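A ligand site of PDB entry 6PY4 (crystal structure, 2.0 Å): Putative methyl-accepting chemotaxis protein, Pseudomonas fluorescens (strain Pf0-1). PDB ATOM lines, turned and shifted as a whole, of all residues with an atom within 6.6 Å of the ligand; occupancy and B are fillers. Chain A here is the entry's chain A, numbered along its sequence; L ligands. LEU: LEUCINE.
Merely in contact with the ligand: Tyr 74 (3.4 Å), Ile 84 (3.9 Å), Met 90 (3.8 Å), Phe 94 (3.6 Å) and Ile 126 (3.5 Å).
Hydrophobic or aromatic side chains that line the ligand: Tyr 74, Ile 84, Met 90, Phe 94, Trp 101, Tyr 117, Ala 120 and Ile 126.
11 residues have an atom within 4 Å of the ligand: Tyr 74, Ile 84, Met 90, Phe 94, Arg 99, Trp 101, Tyr 117, Asp 119, Ala 120, Ile 126 and Asp 146.
The nearest printed residue that does not touch the ligand is Ala 72 (4.04 Å).
The backbone NH of Ala 120 sits at hydrogen-bond distance from an oxygen (OXT) of the ligand (2.8 Å).
N of the ligand is in salt-bridge range of OD2 of Asp 146, at 2.8 Å.
NE of Arg 99 lies within salt-bridge range of O of the ligand, 2.8 Å away.
The indole nitrogen of Trp 101 lies within hydrogen-bond range of an oxygen (O) of the ligand (2.8 Å).
OH of Tyr 117 lies within hydrogen-bond range of N of the ligand (2.9 Å).
The side-chain carboxylate (OD1) of Asp 119 lies within salt-bridge range of a nitrogen (N) of the ligand, 3.1 Å away.
The side-chain hydroxyl (OH) of Tyr 74 is in hydrogen-bond range of the side-chain carboxylate (OD1) of Asp 146, 2.8 Å away.
The backbone carbonyl oxygen of Ala 72 lies within hydrogen-bond range of the backbone NH of Asp 146.
OG of Ser 128 lies within hydrogen-bond range of OD1 of Asp 146.
O of Ile 118 is in hydrogen-bond range of NH2 of Arg 99, 2.9 Å away.
N of Ile 126 sits at hydrogen-bond distance from O of Tyr 117 (2.9 Å).
The side-chain hydroxyl (OG) of Ser 128 is in hydrogen-bond range of the side-chain hydroxyl (OH) of Tyr 117, 2.5 Å away.
The side-chain carboxylate (OD2) of Asp 119 lies within hydrogen-bond range of the side-chain hydroxyl (OG1) of Thr 122 (2.7 Å).
OG of Ser 128 sits at hydrogen-bond distance from OH of Tyr 74, at 3.2 Å.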
ATOM      1  N   ALA A  72      20.012   6.336 -30.657  1.00  0.00           N
ATOM      2  CA  ALA A  72      20.296   7.015 -29.415  1.00  0.00           C
ATOM      3  C   ALA A  72      20.788   5.994 -28.396  1.00  0.00           C
ATOM      4  O   ALA A  72      20.575   4.789 -28.541  1.00  0.00           O
ATOM      5  CB  ALA A  72      19.036   7.710 -28.902  1.00  0.00           C
ATOM      6  N   SER A  73      21.567   6.482 -27.441  1.00  0.00           N
ATOM      7  CA  SER A  73      21.989   5.682 -26.339  1.00  0.00           C
ATOM      8  C   SER A  73      21.634   6.495 -25.112  1.00  0.00           C
ATOM      9  O   SER A  73      21.581   7.745 -25.163  1.00  0.00           O
ATOM     10  CB  SER A  73      23.490   5.382 -26.451  1.00  0.00           C
ATOM     11  OG  SER A  73      24.185   6.601 -26.512  1.00  0.00           O
ATOM     12  N   TYR A  74      21.424   5.811 -23.999  1.00  0.00           N
ATOM     13  CA  TYR A  74      20.800   6.488 -22.862  1.00  0.00           C
ATOM     14  C   TYR A  74      20.953   5.705 -21.602  1.00  0.00           C
ATOM     15  O   TYR A  74      21.272   4.533 -21.655  1.00  0.00           O
ATOM     16  CB  TYR A  74      19.310   6.707 -23.172  1.00  0.00           C
ATOM     17  CG  TYR A  74      18.619   5.497 -23.748  1.00  0.00           C
ATOM     18  CD1 TYR A  74      18.177   4.471 -22.934  1.00  0.00           C
ATOM     19  CD2 TYR A  74      18.466   5.352 -25.103  1.00  0.00           C
ATOM     20  CE1 TYR A  74      17.600   3.331 -23.482  1.00  0.00           C
ATOM     21  CE2 TYR A  74      17.864   4.233 -25.649  1.00  0.00           C
ATOM     22  CZ  TYR A  74      17.457   3.218 -24.814  1.00  0.00           C
ATOM     23  OH  TYR A  74      16.846   2.101 -25.331  1.00  0.00           O
ATOM     24  N   LEU A  75      20.808   6.390 -20.473  1.00  0.00           N
ATOM     25  CA  LEU A  75      20.719   5.775 -19.155  1.00  0.00           C
ATOM     26  C   LEU A  75      19.407   6.259 -18.523  1.00  0.00           C
ATOM     27  O   LEU A  75      19.114   7.465 -18.561  1.00  0.00           O
ATOM     28  CB  LEU A  75      21.905   6.241 -18.270  1.00  0.00           C
ATOM     29  CG  LEU A  75      21.902   5.874 -16.786  1.00  0.00           C
ATOM     30  CD1 LEU A  75      22.104   4.386 -16.582  1.00  0.00           C
ATOM     31  CD2 LEU A  75      22.979   6.647 -16.017  1.00  0.00           C
ATOM     32  N   PHE A  82      16.754  10.464 -16.640  1.00  0.00           N
ATOM     33  CA  PHE A  82      17.284   9.829 -17.828  1.00  0.00           C
ATOM     34  C   PHE A  82      18.230  10.814 -18.518  1.00  0.00           C
ATOM     35  O   PHE A  82      18.003  12.020 -18.466  1.00  0.00           O
ATOM     36  CB  PHE A  82      16.170   9.368 -18.778  1.00  0.00           C
ATOM     37  CG  PHE A  82      15.226  10.461 -19.212  1.00  0.00           C
ATOM     38  CD1 PHE A  82      14.092  10.781 -18.459  1.00  0.00           C
ATOM     39  CD2 PHE A  82      15.442  11.175 -20.381  1.00  0.00           C
ATOM     40  CE1 PHE A  82      13.226  11.779 -18.872  1.00  0.00           C
ATOM     41  CE2 PHE A  82      14.582  12.193 -20.786  1.00  0.00           C
ATOM     42  CZ  PHE A  82      13.488  12.501 -20.006  1.00  0.00           C
ATOM     43  N   THR A  83      19.247  10.280 -19.185  1.00  0.00           N
ATOM     44  CA  THR A  83      20.122  11.043 -20.082  1.00  0.00           C
ATOM     45  C   THR A  83      20.178  10.332 -21.408  1.00  0.00           C
ATOM     46  O   THR A  83      20.402   9.111 -21.432  1.00  0.00           O
ATOM     47  CB  THR A  83      21.541  11.090 -19.509  1.00  0.00           C
ATOM     48  OG1 THR A  83      21.452  11.650 -18.218  1.00  0.00           O
ATOM     49  CG2 THR A  83      22.501  11.931 -20.376  1.00  0.00           C
ATOM     50  N   ILE A  84      19.956  11.097 -22.469  1.00  0.00           N
ATOM     51  CA  ILE A  84      19.875  10.608 -23.814  1.00  0.00           C
ATOM     52  C   ILE A  84      20.829  11.357 -24.736  1.00  0.00           C
ATOM     53  O   ILE A  84      20.814  12.597 -24.788  1.00  0.00           O
ATOM     54  CB  ILE A  84      18.451  10.803 -24.355  1.00  0.00           C
ATOM     55  CG1 ILE A  84      17.421  10.183 -23.403  1.00  0.00           C
ATOM     56  CG2 ILE A  84      18.299  10.210 -25.739  1.00  0.00           C
ATOM     57  CD1 ILE A  84      16.017  10.580 -23.800  1.00  0.00           C
ATOM     58  N   PRO A  86      22.211  11.197 -29.002  1.00  0.00           N
ATOM     59  CA  PRO A  86      21.931  12.643 -29.078  1.00  0.00           C
ATOM     60  C   PRO A  86      20.600  13.014 -28.395  1.00  0.00           C
ATOM     61  O   PRO A  86      19.626  12.244 -28.486  1.00  0.00           O
ATOM     62  CB  PRO A  86      21.824  12.917 -30.584  1.00  0.00           C
ATOM     63  CG  PRO A  86      22.236  11.664 -31.289  1.00  0.00           C
ATOM     64  CD  PRO A  86      22.045  10.539 -30.297  1.00  0.00           C
ATOM     65  N   ALA A  88      17.051  14.202 -27.318  1.00  0.00           N
ATOM     66  CA  ALA A  88      15.780  14.303 -28.037  1.00  0.00           C
ATOM     67  C   ALA A  88      14.679  14.827 -27.106  1.00  0.00           C
ATOM     68  O   ALA A  88      14.722  14.562 -25.902  1.00  0.00           O
ATOM     69  CB  ALA A  88      15.404  12.954 -28.608  1.00  0.00           C
ATOM     70  N   MET A  90      11.506  14.411 -25.403  1.00  0.00           N
ATOM     71  CA  MET A  90      10.658  13.265 -25.036  1.00  0.00           C
ATOM     72  C   MET A  90       9.210  13.690 -24.735  1.00  0.00           C
ATOM     73  O   MET A  90       8.964  14.807 -24.340  1.00  0.00           O
ATOM     74  CB  MET A  90      11.271  12.541 -23.837  1.00  0.00           C
ATOM     75  CG  MET A  90      12.681  12.052 -24.111  1.00  0.00           C
ATOM     76  SD  MET A  90      12.790  11.031 -25.602  1.00  0.00           S
ATOM     77  CE  MET A  90      11.934   9.556 -25.010  1.00  0.00           C
ATOM     78  N   PHE A  94       7.322  11.408 -19.794  1.00  0.00           N
ATOM     79  CA  PHE A  94       8.150  10.244 -20.110  1.00  0.00           C
ATOM     80  C   PHE A  94       8.855   9.699 -18.877  1.00  0.00           C
ATOM     81  O   PHE A  94       9.556  10.430 -18.141  1.00  0.00           O
ATOM     82  CB  PHE A  94       9.155  10.568 -21.203  1.00  0.00           C
ATOM     83  CG  PHE A  94      10.090   9.448 -21.507  1.00  0.00           C
ATOM     84  CD1 PHE A  94       9.678   8.382 -22.304  1.00  0.00           C
ATOM     85  CD2 PHE A  94      11.377   9.438 -20.982  1.00  0.00           C
ATOM     86  CE1 PHE A  94      10.542   7.339 -22.573  1.00  0.00           C
ATOM     87  CE2 PHE A  94      12.252   8.400 -21.272  1.00  0.00           C
ATOM     88  CZ  PHE A  94      11.829   7.330 -22.062  1.00  0.00           C
ATOM     89  N   ASP A  95       8.657   8.407 -18.622  1.00  0.00           N
ATOM     90  CA  ASP A  95       9.282   7.733 -17.471  1.00  0.00           C
ATOM     91  C   ASP A  95      10.016   6.486 -17.987  1.00  0.00           C
ATOM     92  O   ASP A  95       9.378   5.566 -18.465  1.00  0.00           O
ATOM     93  CB  ASP A  95       8.217   7.318 -16.445  1.00  0.00           C
ATOM     94  CG  ASP A  95       8.795   6.645 -15.186  1.00  0.00           C
ATOM     95  OD1 ASP A  95      10.017   6.391 -15.081  1.00  0.00           O
ATOM     96  OD2 ASP A  95       8.016   6.375 -14.232  1.00  0.00           O
ATOM     97  N   PRO A  96      11.357   6.442 -17.897  1.00  0.00           N
ATOM     98  CA  PRO A  96      12.087   5.292 -18.430  1.00  0.00           C
ATOM     99  C   PRO A  96      11.755   4.004 -17.703  1.00  0.00           C
ATOM    100  O   PRO A  96      11.850   2.936 -18.290  1.00  0.00           O
ATOM    101  CB  PRO A  96      13.557   5.654 -18.176  1.00  0.00           C
ATOM    102  CG  PRO A  96      13.515   6.513 -16.971  1.00  0.00           C
ATOM    103  CD  PRO A  96      12.267   7.374 -17.208  1.00  0.00           C
ATOM    104  N   ARG A  99       9.289   1.629 -19.469  1.00  0.00           N
ATOM    105  CA  ARG A  99       9.529   1.296 -20.867  1.00  0.00           C
ATOM    106  C   ARG A  99      10.096  -0.125 -21.033  1.00  0.00           C
ATOM    107  O   ARG A  99      10.683  -0.677 -20.087  1.00  0.00           O
ATOM    108  CB  ARG A  99      10.495   2.336 -21.435  1.00  0.00           C
ATOM    109  CG  ARG A  99       9.977   3.760 -21.342  1.00  0.00           C
ATOM    110  CD  ARG A  99       8.740   3.968 -22.192  1.00  0.00           C
ATOM    111  NE  ARG A  99       9.041   3.787 -23.606  1.00  0.00           N
ATOM    112  CZ  ARG A  99       8.114   3.625 -24.534  1.00  0.00           C
ATOM    113  NH1 ARG A  99       6.851   3.424 -24.156  1.00  0.00           N
ATOM    114  NH2 ARG A  99       8.442   3.557 -25.822  1.00  0.00           N
ATOM    115  N   PRO A 100       9.924  -0.750 -22.205  1.00  0.00           N
ATOM    116  CA  PRO A 100      10.306  -2.173 -22.315  1.00  0.00           C
ATOM    117  C   PRO A 100      11.805  -2.482 -22.186  1.00  0.00           C
ATOM    118  O   PRO A 100      12.188  -3.547 -21.712  1.00  0.00           O
ATOM    119  CB  PRO A 100       9.781  -2.610 -23.701  1.00  0.00           C
ATOM    120  CG  PRO A 100       9.334  -1.365 -24.398  1.00  0.00           C
ATOM    121  CD  PRO A 100       9.146  -0.290 -23.369  1.00  0.00           C
ATOM    122  N   TRP A 101      12.643  -1.551 -22.621  1.00  0.00           N
ATOM    123  CA  TRP A 101      14.080  -1.749 -22.478  1.00  0.00           C
ATOM    124  C   TRP A 101      14.455  -1.794 -21.004  1.00  0.00           C
ATOM    125  O   TRP A 101      15.355  -2.551 -20.609  1.00  0.00           O
ATOM    126  CB  TRP A 101      14.838  -0.644 -23.220  1.00  0.00           C
ATOM    127  CG  TRP A 101      14.479   0.784 -22.848  1.00  0.00           C
ATOM    128  CD1 TRP A 101      13.522   1.549 -23.411  1.00  0.00           C
ATOM    129  CD2 TRP A 101      15.103   1.607 -21.857  1.00  0.00           C
ATOM    130  NE1 TRP A 101      13.486   2.798 -22.839  1.00  0.00           N
ATOM    131  CE2 TRP A 101      14.448   2.853 -21.868  1.00  0.00           C
ATOM    132  CE3 TRP A 101      16.160   1.418 -20.958  1.00  0.00           C
ATOM    133  CZ2 TRP A 101      14.839   3.917 -21.063  1.00  0.00           C
ATOM    134  CZ3 TRP A 101      16.545   2.462 -20.162  1.00  0.00           C
ATOM    135  CH2 TRP A 101      15.886   3.696 -20.201  1.00  0.00           C
ATOM    136  N   TYR A 117       9.127  -2.435 -30.528  1.00  0.00           N
ATOM    137  CA  TYR A 117       8.151  -1.606 -29.819  1.00  0.00           C
ATOM    138  C   TYR A 117       8.211  -0.224 -30.455  1.00  0.00           C
ATOM    139  O   TYR A 117       9.117   0.063 -31.242  1.00  0.00           O
ATOM    140  CB  TYR A 117       8.444  -1.541 -28.324  1.00  0.00           C
ATOM    141  CG  TYR A 117       9.753  -0.848 -27.920  1.00  0.00           C
ATOM    142  CD1 TYR A 117      10.989  -1.482 -27.962  1.00  0.00           C
ATOM    143  CD2 TYR A 117       9.738   0.451 -27.425  1.00  0.00           C
ATOM    144  CE1 TYR A 117      12.169  -0.841 -27.558  1.00  0.00           C
ATOM    145  CE2 TYR A 117      10.893   1.077 -27.027  1.00  0.00           C
ATOM    146  CZ  TYR A 117      12.128   0.445 -27.111  1.00  0.00           C
ATOM    147  OH  TYR A 117      13.271   1.150 -26.766  1.00  0.00           O
ATOM    148  N   ILE A 118       7.295   0.645 -30.058  1.00  0.00           N
ATOM    149  CA  ILE A 118       7.231   2.013 -30.605  1.00  0.00           C
ATOM    150  C   ILE A 118       8.130   2.968 -29.850  1.00  0.00           C
ATOM    151  O   ILE A 118       7.955   3.233 -28.670  1.00  0.00           O
ATOM    152  CB  ILE A 118       5.806   2.569 -30.603  1.00  0.00           C
ATOM    153  CG1 ILE A 118       4.920   1.582 -31.360  1.00  0.00           C
ATOM    154  CG2 ILE A 118       5.791   3.969 -31.179  1.00  0.00           C
ATOM    155  CD1 ILE A 118       3.425   1.773 -31.141  1.00  0.00           C
ATOM    156  N   ASP A 119       9.127   3.498 -30.536  1.00  0.00           N
ATOM    157  CA  ASP A 119      10.087   4.433 -29.904  1.00  0.00           C
ATOM    158  C   ASP A 119       9.451   5.687 -29.327  1.00  0.00           C
ATOM    159  O   ASP A 119       8.698   6.350 -30.036  1.00  0.00           O
ATOM    160  CB  ASP A 119      11.143   4.822 -30.960  1.00  0.00           C
ATOM    161  CG  ASP A 119      12.251   5.705 -30.407  1.00  0.00           C
ATOM    162  OD1 ASP A 119      12.388   5.771 -29.168  1.00  0.00           O
ATOM    163  OD2 ASP A 119      12.950   6.345 -31.240  1.00  0.00           O
ATOM    164  N   ALA A 120       9.700   6.008 -28.059  1.00  0.00           N
ATOM    165  CA  ALA A 120       9.151   7.238 -27.485  1.00  0.00           C
ATOM    166  C   ALA A 120       9.735   8.490 -28.130  1.00  0.00           C
ATOM    167  O   ALA A 120       9.176   9.573 -28.024  1.00  0.00           O
ATOM    168  CB  ALA A 120       9.368   7.331 -25.979  1.00  0.00           C
ATOM    169  N   ALA A 121      10.963   8.389 -28.598  1.00  0.00           N
ATOM    170  CA  ALA A 121      11.647   9.511 -29.238  1.00  0.00           C
ATOM    171  C   ALA A 121      11.115   9.765 -30.633  1.00  0.00           C
ATOM    172  O   ALA A 121      10.581  10.812 -30.898  1.00  0.00           O
ATOM    173  CB  ALA A 121      13.146   9.267 -29.291  1.00  0.00           C
ATOM    174  N   THR A 122      11.247   8.811 -31.548  1.00  0.00           N
ATOM    175  CA  THR A 122      10.949   9.089 -32.948  1.00  0.00           C
ATOM    176  C   THR A 122       9.574   8.648 -33.351  1.00  0.00           C
ATOM    177  O   THR A 122       9.170   8.944 -34.464  1.00  0.00           O
ATOM    178  CB  THR A 122      11.908   8.309 -33.860  1.00  0.00           C
ATOM    179  OG1 THR A 122      11.729   6.903 -33.632  1.00  0.00           O
ATOM    180  CG2 THR A 122      13.351   8.714 -33.567  1.00  0.00           C
ATOM    181  N   ILE A 126      11.187   0.080 -33.311  1.00  0.00           N
ATOM    182  CA  ILE A 126      12.592  -0.107 -33.017  1.00  0.00           C
ATOM    183  C   ILE A 126      12.803  -1.367 -32.172  1.00  0.00           C
ATOM    184  O   ILE A 126      11.858  -1.914 -31.609  1.00  0.00           O
ATOM    185  CB  ILE A 126      13.216   1.101 -32.298  1.00  0.00           C
ATOM    186  CG1 ILE A 126      12.581   1.325 -30.936  1.00  0.00           C
ATOM    187  CG2 ILE A 126      13.137   2.390 -33.139  1.00  0.00           C
ATOM    188  CD1 ILE A 126      13.419   2.142 -30.001  1.00  0.00           C
ATOM    189  N   SER A 128      15.704  -2.409 -28.936  1.00  0.00           N
ATOM    190  CA  SER A 128      16.762  -1.824 -28.134  1.00  0.00           C
ATOM    191  C   SER A 128      17.597  -2.958 -27.564  1.00  0.00           C
ATOM    192  O   SER A 128      17.079  -4.034 -27.203  1.00  0.00           O
ATOM    193  CB  SER A 128      16.213  -1.028 -26.972  1.00  0.00           C
ATOM    194  OG  SER A 128      15.453   0.060 -27.441  1.00  0.00           O
ATOM    195  N   GLY A 145      20.516   1.181 -26.052  1.00  0.00           N
ATOM    196  CA  GLY A 145      20.702   1.806 -27.352  1.00  0.00           C
ATOM    197  C   GLY A 145      19.651   1.313 -28.320  1.00  0.00           C
ATOM    198  O   GLY A 145      19.269   0.148 -28.301  1.00  0.00           O
ATOM    199  N   ASP A 146      19.258   2.185 -29.221  1.00  0.00           N
ATOM    200  CA  ASP A 146      18.171   1.889 -30.108  1.00  0.00           C
ATOM    201  C   ASP A 146      18.669   1.588 -31.512  1.00  0.00           C
ATOM    202  O   ASP A 146      19.531   2.316 -32.007  1.00  0.00           O
ATOM    203  CB  ASP A 146      17.259   3.113 -30.175  1.00  0.00           C
ATOM    204  CG  ASP A 146      16.495   3.332 -28.893  1.00  0.00           C
ATOM    205  OD1 ASP A 146      16.446   2.381 -28.081  1.00  0.00           O
ATOM    206  OD2 ASP A 146      16.007   4.473 -28.709  1.00  0.00           O
HETATM  207  N   LEU L   1      13.785   4.016 -27.081  1.00  0.00           N
HETATM  208  CA  LEU L   1      13.466   4.731 -25.846  1.00  0.00           C
HETATM  209  C   LEU L   1      11.993   4.485 -25.493  1.00  0.00           C
HETATM  210  O   LEU L   1      11.690   4.397 -24.305  1.00  0.00           O
HETATM  211  CB  LEU L   1      13.618   6.251 -25.989  1.00  0.00           C
HETATM  212  CG  LEU L   1      14.771   7.070 -25.433  1.00  0.00           C
HETATM  213  CD1 LEU L   1      15.794   7.380 -26.506  1.00  0.00           C
HETATM  214  CD2 LEU L   1      15.393   6.552 -24.133  1.00  0.00           C
HETATM  215  OXT LEU L   1      11.130   4.363 -26.378  1.00  0.00           O
